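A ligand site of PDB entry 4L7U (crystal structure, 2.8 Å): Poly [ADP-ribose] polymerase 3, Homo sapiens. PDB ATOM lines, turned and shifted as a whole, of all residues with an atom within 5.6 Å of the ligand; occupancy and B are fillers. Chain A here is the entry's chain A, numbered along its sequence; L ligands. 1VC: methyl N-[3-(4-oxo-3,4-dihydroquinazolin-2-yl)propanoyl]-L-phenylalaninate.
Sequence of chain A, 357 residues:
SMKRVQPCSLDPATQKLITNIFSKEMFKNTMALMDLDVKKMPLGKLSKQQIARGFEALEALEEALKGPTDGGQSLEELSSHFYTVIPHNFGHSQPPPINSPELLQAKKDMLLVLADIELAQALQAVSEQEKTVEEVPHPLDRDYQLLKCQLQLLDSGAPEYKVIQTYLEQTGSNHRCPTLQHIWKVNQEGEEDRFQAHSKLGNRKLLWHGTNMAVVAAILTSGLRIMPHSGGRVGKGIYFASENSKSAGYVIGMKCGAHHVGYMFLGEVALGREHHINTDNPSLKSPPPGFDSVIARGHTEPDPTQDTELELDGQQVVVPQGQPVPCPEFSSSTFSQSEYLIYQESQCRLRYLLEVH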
ATOM      1  N   ASP A 109      11.765 -37.662 -21.083  1.00  0.00           N
ATOM      2  CA  ASP A 109      11.216 -37.043 -22.284  1.00  0.00           C
ATOM      3  C   ASP A 109      10.317 -38.035 -23.086  1.00  0.00           C
ATOM      4  O   ASP A 109       9.436 -37.607 -23.820  1.00  0.00           O
ATOM      5  CB  ASP A 109      12.351 -36.428 -23.152  1.00  0.00           C
ATOM      6  CG  ASP A 109      13.062 -35.205 -22.543  1.00  0.00           C
ATOM      7  OD1 ASP A 109      12.469 -34.550 -21.634  1.00  0.00           O
ATOM      8  OD2 ASP A 109      14.206 -34.903 -22.970  1.00  0.00           O
ATOM      9  N   LEU A 112       7.000 -37.768 -21.163  1.00  0.00           N
ATOM     10  CA  LEU A 112       6.372 -36.484 -21.445  1.00  0.00           C
ATOM     11  C   LEU A 112       5.597 -36.540 -22.775  1.00  0.00           C
ATOM     12  O   LEU A 112       4.710 -35.722 -22.994  1.00  0.00           O
ATOM     13  CB  LEU A 112       7.389 -35.316 -21.479  1.00  0.00           C
ATOM     14  CG  LEU A 112       8.013 -34.826 -20.138  1.00  0.00           C
ATOM     15  CD1 LEU A 112       8.962 -33.666 -20.378  1.00  0.00           C
ATOM     16  CD2 LEU A 112       6.939 -34.405 -19.120  1.00  0.00           C
ATOM     17  N   VAL A 113       5.947 -37.481 -23.671  1.00  0.00           N
ATOM     18  CA  VAL A 113       5.249 -37.651 -24.938  1.00  0.00           C
ATOM     19  C   VAL A 113       4.021 -38.519 -24.660  1.00  0.00           C
ATOM     20  O   VAL A 113       2.912 -38.131 -25.008  1.00  0.00           O
ATOM     21  CB  VAL A 113       6.151 -38.219 -26.087  1.00  0.00           C
ATOM     22  CG1 VAL A 113       5.339 -38.571 -27.332  1.00  0.00           C
ATOM     23  CG2 VAL A 113       7.252 -37.229 -26.438  1.00  0.00           C
ATOM     24  N   ASP A 116       0.981 -36.816 -23.318  1.00  0.00           N
ATOM     25  CA  ASP A 116       0.255 -36.114 -24.371  1.00  0.00           C
ATOM     26  C   ASP A 116      -0.480 -37.129 -25.262  1.00  0.00           C
ATOM     27  O   ASP A 116      -1.517 -36.800 -25.852  1.00  0.00           O
ATOM     28  CB  ASP A 116       1.206 -35.232 -25.207  1.00  0.00           C
ATOM     29  CG  ASP A 116       1.860 -34.098 -24.442  1.00  0.00           C
ATOM     30  OD1 ASP A 116       1.982 -34.196 -23.196  1.00  0.00           O
ATOM     31  OD2 ASP A 116       2.273 -33.110 -25.085  1.00  0.00           O
ATOM     32  N   TRP A 208      10.312 -20.613 -34.015  1.00  0.00           N
ATOM     33  CA  TRP A 208       9.917 -22.001 -34.286  1.00  0.00           C
ATOM     34  C   TRP A 208       9.801 -22.803 -33.006  1.00  0.00           C
ATOM     35  O   TRP A 208      10.258 -22.358 -31.947  1.00  0.00           O
ATOM     36  CB  TRP A 208      10.924 -22.713 -35.219  1.00  0.00           C
ATOM     37  CG  TRP A 208      11.144 -22.069 -36.553  1.00  0.00           C
ATOM     38  CD1 TRP A 208      12.252 -21.383 -36.941  1.00  0.00           C
ATOM     39  CD2 TRP A 208      10.260 -22.067 -37.677  1.00  0.00           C
ATOM     40  NE1 TRP A 208      12.118 -20.955 -38.238  1.00  0.00           N
ATOM     41  CE2 TRP A 208      10.896 -21.347 -38.712  1.00  0.00           C
ATOM     42  CE3 TRP A 208       8.978 -22.597 -37.908  1.00  0.00           C
ATOM     43  CZ2 TRP A 208      10.295 -21.136 -39.957  1.00  0.00           C
ATOM     44  CZ3 TRP A 208       8.389 -22.408 -39.151  1.00  0.00           C
ATOM     45  CH2 TRP A 208       9.041 -21.675 -40.158  1.00  0.00           C
ATOM     46  N   HIS A 209       9.221 -24.019 -33.134  1.00  0.00           N
ATOM     47  CA  HIS A 209       9.033 -25.035 -32.096  1.00  0.00           C
ATOM     48  C   HIS A 209       8.602 -26.328 -32.799  1.00  0.00           C
ATOM     49  O   HIS A 209       7.559 -26.375 -33.415  1.00  0.00           O
ATOM     50  CB  HIS A 209       8.003 -24.590 -31.042  1.00  0.00           C
ATOM     51  CG  HIS A 209       7.970 -25.501 -29.862  1.00  0.00           C
ATOM     52  ND1 HIS A 209       8.701 -25.230 -28.734  1.00  0.00           N
ATOM     53  CD2 HIS A 209       7.336 -26.685 -29.704  1.00  0.00           C
ATOM     54  CE1 HIS A 209       8.488 -26.256 -27.933  1.00  0.00           C
ATOM     55  NE2 HIS A 209       7.673 -27.153 -28.469  1.00  0.00           N
ATOM     56  N   GLY A 210       9.465 -27.319 -32.746  1.00  0.00           N
ATOM     57  CA  GLY A 210       9.262 -28.612 -33.392  1.00  0.00           C
ATOM     58  C   GLY A 210       8.958 -29.720 -32.413  1.00  0.00           C
ATOM     59  O   GLY A 210       9.600 -29.833 -31.375  1.00  0.00           O
ATOM     60  N   THR A 211       7.964 -30.549 -32.763  1.00  0.00           N
ATOM     61  CA  THR A 211       7.485 -31.661 -31.938  1.00  0.00           C
ATOM     62  C   THR A 211       7.141 -32.858 -32.802  1.00  0.00           C
ATOM     63  O   THR A 211       6.944 -32.666 -34.010  1.00  0.00           O
ATOM     64  CB  THR A 211       6.204 -31.221 -31.186  1.00  0.00           C
ATOM     65  OG1 THR A 211       5.282 -30.622 -32.099  1.00  0.00           O
ATOM     66  CG2 THR A 211       6.475 -30.283 -30.037  1.00  0.00           C
ATOM     67  N   ASN A 212       7.001 -34.071 -32.201  1.00  0.00           N
ATOM     68  CA  ASN A 212       6.530 -35.205 -32.978  1.00  0.00           C
ATOM     69  C   ASN A 212       4.961 -35.200 -32.974  1.00  0.00           C
ATOM     70  O   ASN A 212       4.336 -34.778 -31.996  1.00  0.00           O
ATOM     71  CB  ASN A 212       7.139 -36.550 -32.538  1.00  0.00           C
ATOM     72  CG  ASN A 212       6.818 -37.063 -31.161  1.00  0.00           C
ATOM     73  OD1 ASN A 212       5.692 -37.422 -30.847  1.00  0.00           O
ATOM     74  ND2 ASN A 212       7.849 -37.264 -30.360  1.00  0.00           N
ATOM     75  N   VAL A 215       1.972 -35.146 -29.998  1.00  0.00           N
ATOM     76  CA  VAL A 215       1.870 -34.138 -28.937  1.00  0.00           C
ATOM     77  C   VAL A 215       1.190 -32.852 -29.495  1.00  0.00           C
ATOM     78  O   VAL A 215       0.798 -31.979 -28.708  1.00  0.00           O
ATOM     79  CB  VAL A 215       3.207 -33.821 -28.227  1.00  0.00           C
ATOM     80  CG1 VAL A 215       3.820 -35.042 -27.567  1.00  0.00           C
ATOM     81  CG2 VAL A 215       4.194 -33.166 -29.163  1.00  0.00           C
ATOM     82  N   ILE A 219      -0.856 -29.748 -27.547  1.00  0.00           N
ATOM     83  CA  ILE A 219      -0.466 -28.326 -27.655  1.00  0.00           C
ATOM     84  C   ILE A 219      -1.679 -27.524 -28.229  1.00  0.00           C
ATOM     85  O   ILE A 219      -1.981 -26.433 -27.757  1.00  0.00           O
ATOM     86  CB  ILE A 219       0.874 -28.094 -28.432  1.00  0.00           C
ATOM     87  CG1 ILE A 219       2.042 -28.747 -27.684  1.00  0.00           C
ATOM     88  CG2 ILE A 219       1.177 -26.605 -28.647  1.00  0.00           C
ATOM     89  CD1 ILE A 219       3.085 -29.410 -28.538  1.00  0.00           C
ATOM     90  N   TYR A 239      11.408 -24.421 -25.116  1.00  0.00           N
ATOM     91  CA  TYR A 239      12.494 -24.335 -26.104  1.00  0.00           C
ATOM     92  C   TYR A 239      12.049 -23.850 -27.491  1.00  0.00           C
ATOM     93  O   TYR A 239      11.203 -24.467 -28.122  1.00  0.00           O
ATOM     94  CB  TYR A 239      13.194 -25.708 -26.220  1.00  0.00           C
ATOM     95  CG  TYR A 239      14.057 -26.046 -25.019  1.00  0.00           C
ATOM     96  CD1 TYR A 239      15.437 -25.866 -25.059  1.00  0.00           C
ATOM     97  CD2 TYR A 239      13.494 -26.550 -23.849  1.00  0.00           C
ATOM     98  CE1 TYR A 239      16.235 -26.171 -23.956  1.00  0.00           C
ATOM     99  CE2 TYR A 239      14.277 -26.832 -22.725  1.00  0.00           C
ATOM    100  CZ  TYR A 239      15.649 -26.646 -22.785  1.00  0.00           C
ATOM    101  OH  TYR A 239      16.436 -26.921 -21.702  1.00  0.00           O
ATOM    102  N   PHE A 240      12.674 -22.737 -27.967  1.00  0.00           N
ATOM    103  CA  PHE A 240      12.473 -22.128 -29.296  1.00  0.00           C
ATOM    104  C   PHE A 240      13.809 -21.890 -30.038  1.00  0.00           C
ATOM    105  O   PHE A 240      14.790 -21.442 -29.453  1.00  0.00           O
ATOM    106  CB  PHE A 240      11.729 -20.793 -29.210  1.00  0.00           C
ATOM    107  CG  PHE A 240      10.410 -20.800 -28.485  1.00  0.00           C
ATOM    108  CD1 PHE A 240       9.227 -21.090 -29.153  1.00  0.00           C
ATOM    109  CD2 PHE A 240      10.339 -20.432 -27.139  1.00  0.00           C
ATOM    110  CE1 PHE A 240       8.012 -21.084 -28.471  1.00  0.00           C
ATOM    111  CE2 PHE A 240       9.121 -20.387 -26.473  1.00  0.00           C
ATOM    112  CZ  PHE A 240       7.964 -20.732 -27.130  1.00  0.00           C
ATOM    113  N   ALA A 241      13.793 -22.140 -31.358  1.00  0.00           N
ATOM    114  CA  ALA A 241      14.924 -21.909 -32.256  1.00  0.00           C
ATOM    115  C   ALA A 241      14.583 -20.872 -33.280  1.00  0.00           C
ATOM    116  O   ALA A 241      13.453 -20.882 -33.786  1.00  0.00           O
ATOM    117  CB  ALA A 241      15.291 -23.190 -32.953  1.00  0.00           C
ATOM    118  N   LYS A 246      17.218 -26.576 -36.560  1.00  0.00           N
ATOM    119  CA  LYS A 246      17.232 -26.964 -35.121  1.00  0.00           C
ATOM    120  C   LYS A 246      15.896 -27.525 -34.623  1.00  0.00           C
ATOM    121  O   LYS A 246      15.874 -28.575 -33.976  1.00  0.00           O
ATOM    122  CB  LYS A 246      17.654 -25.797 -34.211  1.00  0.00           C
ATOM    123  CG  LYS A 246      17.636 -26.140 -32.709  1.00  0.00           C
ATOM    124  CD  LYS A 246      18.762 -27.100 -32.309  1.00  0.00           C
ATOM    125  CE  LYS A 246      18.588 -27.659 -30.924  1.00  0.00           C
ATOM    126  NZ  LYS A 246      19.678 -28.598 -30.583  1.00  0.00           N
ATOM    127  N   SER A 247      14.789 -26.846 -34.906  1.00  0.00           N
ATOM    128  CA  SER A 247      13.453 -27.326 -34.493  1.00  0.00           C
ATOM    129  C   SER A 247      13.025 -28.624 -35.208  1.00  0.00           C
ATOM    130  O   SER A 247      12.539 -29.541 -34.527  1.00  0.00           O
ATOM    131  CB  SER A 247      12.429 -26.236 -34.752  1.00  0.00           C
ATOM    132  OG  SER A 247      12.660 -25.179 -33.837  1.00  0.00           O
ATOM    133  N   TYR A 250      13.503 -32.567 -34.153  1.00  0.00           N
ATOM    134  CA  TYR A 250      12.556 -33.149 -33.193  1.00  0.00           C
ATOM    135  C   TYR A 250      11.244 -33.650 -33.852  1.00  0.00           C
ATOM    136  O   TYR A 250      10.449 -34.368 -33.231  1.00  0.00           O
ATOM    137  CB  TYR A 250      12.226 -32.106 -32.118  1.00  0.00           C
ATOM    138  CG  TYR A 250      13.473 -31.636 -31.388  1.00  0.00           C
ATOM    139  CD1 TYR A 250      14.013 -32.385 -30.344  1.00  0.00           C
ATOM    140  CD2 TYR A 250      14.146 -30.482 -31.788  1.00  0.00           C
ATOM    141  CE1 TYR A 250      15.176 -31.991 -29.697  1.00  0.00           C
ATOM    142  CE2 TYR A 250      15.308 -30.074 -31.146  1.00  0.00           C
ATOM    143  CZ  TYR A 250      15.815 -30.813 -30.088  1.00  0.00           C
ATOM    144  OH  TYR A 250      16.966 -30.415 -29.429  1.00  0.00           O
ATOM    145  N   VAL A 251      11.050 -33.254 -35.123  1.00  0.00           N
ATOM    146  CA  VAL A 251       9.886 -33.601 -35.903  1.00  0.00           C
ATOM    147  C   VAL A 251      10.216 -34.883 -36.635  1.00  0.00           C
ATOM    148  O   VAL A 251      10.928 -34.882 -37.637  1.00  0.00           O
ATOM    149  CB  VAL A 251       9.405 -32.459 -36.865  1.00  0.00           C
ATOM    150  CG1 VAL A 251       7.975 -32.706 -37.340  1.00  0.00           C
ATOM    151  CG2 VAL A 251       9.507 -31.073 -36.216  1.00  0.00           C
ATOM    152  N   SER A 338      21.253 -21.095 -32.024  1.00  0.00           N
ATOM    153  CA  SER A 338      20.597 -20.452 -30.883  1.00  0.00           C
ATOM    154  C   SER A 338      19.378 -21.253 -30.377  1.00  0.00           C
ATOM    155  O   SER A 338      18.683 -21.915 -31.152  1.00  0.00           O
ATOM    156  CB  SER A 338      20.190 -19.022 -31.219  1.00  0.00           C
ATOM    157  OG  SER A 338      21.336 -18.257 -31.570  1.00  0.00           O
ATOM    158  N   GLU A 339      19.172 -21.197 -29.047  1.00  0.00           N
ATOM    159  CA  GLU A 339      18.094 -21.798 -28.267  1.00  0.00           C
ATOM    160  C   GLU A 339      17.514 -20.709 -27.361  1.00  0.00           C
ATOM    161  O   GLU A 339      18.275 -20.089 -26.591  1.00  0.00           O
ATOM    162  CB  GLU A 339      18.589 -23.014 -27.458  1.00  0.00           C
ATOM    163  CG  GLU A 339      18.975 -24.199 -28.341  1.00  0.00           C
ATOM    164  CD  GLU A 339      19.498 -25.451 -27.666  1.00  0.00           C
ATOM    165  OE1 GLU A 339      19.160 -25.701 -26.491  1.00  0.00           O
ATOM    166  OE2 GLU A 339      20.222 -26.211 -28.363  1.00  0.00           O
ATOM    167  N   TYR A 340      16.202 -20.431 -27.484  1.00  0.00           N
ATOM    168  CA  TYR A 340      15.482 -19.375 -26.754  1.00  0.00           C
ATOM    169  C   TYR A 340      14.610 -20.002 -25.690  1.00  0.00           C
ATOM    170  O   TYR A 340      13.752 -20.815 -26.003  1.00  0.00           O
ATOM    171  CB  TYR A 340      14.638 -18.505 -27.727  1.00  0.00           C
ATOM    172  CG  TYR A 340      15.445 -17.823 -28.814  1.00  0.00           C
ATOM    173  CD1 TYR A 340      15.674 -16.455 -28.781  1.00  0.00           C
ATOM    174  CD2 TYR A 340      15.951 -18.541 -29.887  1.00  0.00           C
ATOM    175  CE1 TYR A 340      16.436 -15.826 -29.763  1.00  0.00           C
ATOM    176  CE2 TYR A 340      16.715 -17.917 -30.882  1.00  0.00           C
ATOM    177  CZ  TYR A 340      16.932 -16.563 -30.822  1.00  0.00           C
ATOM    178  OH  TYR A 340      17.666 -15.946 -31.811  1.00  0.00           O
HETATM  179  CD1 1VC L   1       7.452 -33.771 -25.545  1.00  0.00           C
HETATM  180  CE1 1VC L   1       6.125 -33.478 -25.257  1.00  0.00           C
HETATM  181  CZ  1VC L   1       5.762 -32.175 -25.010  1.00  0.00           C
HETATM  182  CE2 1VC L   1       6.727 -31.166 -25.053  1.00  0.00           C
HETATM  183  CD2 1VC L   1       8.053 -31.472 -25.315  1.00  0.00           C
HETATM  184  CG  1VC L   1       8.388 -32.783 -25.577  1.00  0.00           C
HETATM  185  CB  1VC L   1       9.594 -33.157 -25.876  1.00  0.00           C
HETATM  186  CA  1VC L   1       9.798 -32.921 -27.394  1.00  0.00           C
HETATM  187  C   1VC L   1       8.972 -33.166 -28.713  1.00  0.00           C
HETATM  188  O   1VC L   1       9.625 -33.382 -29.794  1.00  0.00           O
HETATM  189  OAT 1VC L   1       7.602 -33.147 -28.692  1.00  0.00           O
HETATM  190  CAA 1VC L   1       7.149 -34.495 -28.927  1.00  0.00           C
HETATM  191  N   1VC L   1      10.410 -31.644 -27.544  1.00  0.00           N
HETATM  192  CAU 1VC L   1       9.836 -30.485 -27.824  1.00  0.00           C
HETATM  193  OAB 1VC L   1       8.672 -30.191 -28.031  1.00  0.00           O
HETATM  194  CAN 1VC L   1      10.757 -29.411 -27.906  1.00  0.00           C
HETATM  195  CAO 1VC L   1      11.648 -29.833 -29.012  1.00  0.00           C
HETATM  196  CAX 1VC L   1      12.332 -28.794 -29.298  1.00  0.00           C
HETATM  197  NAQ 1VC L   1      13.457 -28.661 -28.595  1.00  0.00           N
HETATM  198  CAZ 1VC L   1      14.216 -27.630 -28.913  1.00  0.00           C
HETATM  199  CAL 1VC L   1      15.395 -27.523 -28.208  1.00  0.00           C
HETATM  200  CAH 1VC L   1      16.232 -26.465 -28.532  1.00  0.00           C
HETATM  201  CAI 1VC L   1      15.911 -25.551 -29.522  1.00  0.00           C
HETATM  202  CAM 1VC L   1      14.708 -25.671 -30.180  1.00  0.00           C
HETATM  203  CBA 1VC L   1      13.854 -26.693 -29.918  1.00  0.00           C
HETATM  204  CAY 1VC L   1      12.639 -26.818 -30.645  1.00  0.00           C
HETATM  205  OAD 1VC L   1      12.247 -26.026 -31.507  1.00  0.00           O
HETATM  206  NAS 1VC L   1      11.868 -27.914 -30.334  1.00  0.00           N
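The side-chain hydroxyl (OG) of Ser 247 sits at hydrogen-bond distance from an oxygen (OAD) of the ligand, at 2.5 Å. An oxygen (OAD) of the ligand lies within hydrogen-bond range of the backbone NH (N) of Gly 210 (3.3 Å). O of Gly 210 lies close to NAS of the ligand (3.1 Å). NE2 of His 209 is in hydrogen-bond range of OAB of the ligand, at 3.2 Å.
A ring nitrogen (ND1) of His 209 is in hydrogen-bond range of the backbone carbonyl oxygen (O) of Tyr 239, at 2.7 Å. OH of Tyr 250 sits at hydrogen-bond distance from NZ of Lys 246 (3.5 Å). The side-chain carboxylate (OE2) of Glu 339 lies within salt-bridge range of the side-chain amino group (NZ) of Lys 246 (3.3 Å). The backbone carbonyl oxygen of Ala 241 is in hydrogen-bond range of the backbone NH of Trp 208 (3.2 Å). N of Tyr 340 sits at hydrogen-bond distance from O of Phe 240 (2.6 Å).
Leu 112 touches the ligand. Val 113 touches the ligand. OD2 of Asp 116 touches CZ of the ligand, 3.6 Å away. Thr 211 touches the ligand (CG2 to OAB, 3.0 Å). Asn 212 touches the ligand (ND2 to CAA, 3.2 Å). Val 215 touches the ligand. Tyr 239 touches the ligand (CB to CAZ, 3.5 Å). Phe 240 touches the ligand (C to CAM, 3.9 Å). Ala 241 touches the ligand. CE of Lys 246 touches CAH of the ligand (3.6 Å). Tyr 250 touches the ligand (CE2 to NAQ, 3.5 Å). Glu 339 touches the ligand. Hydrophobic or aromatic side chains that line the ligand: Val 113, His 209, Val 215, Tyr 239, Ala 241 and Tyr 250. Of the 21 residues printed, 15 come within 4 Å of the ligand.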
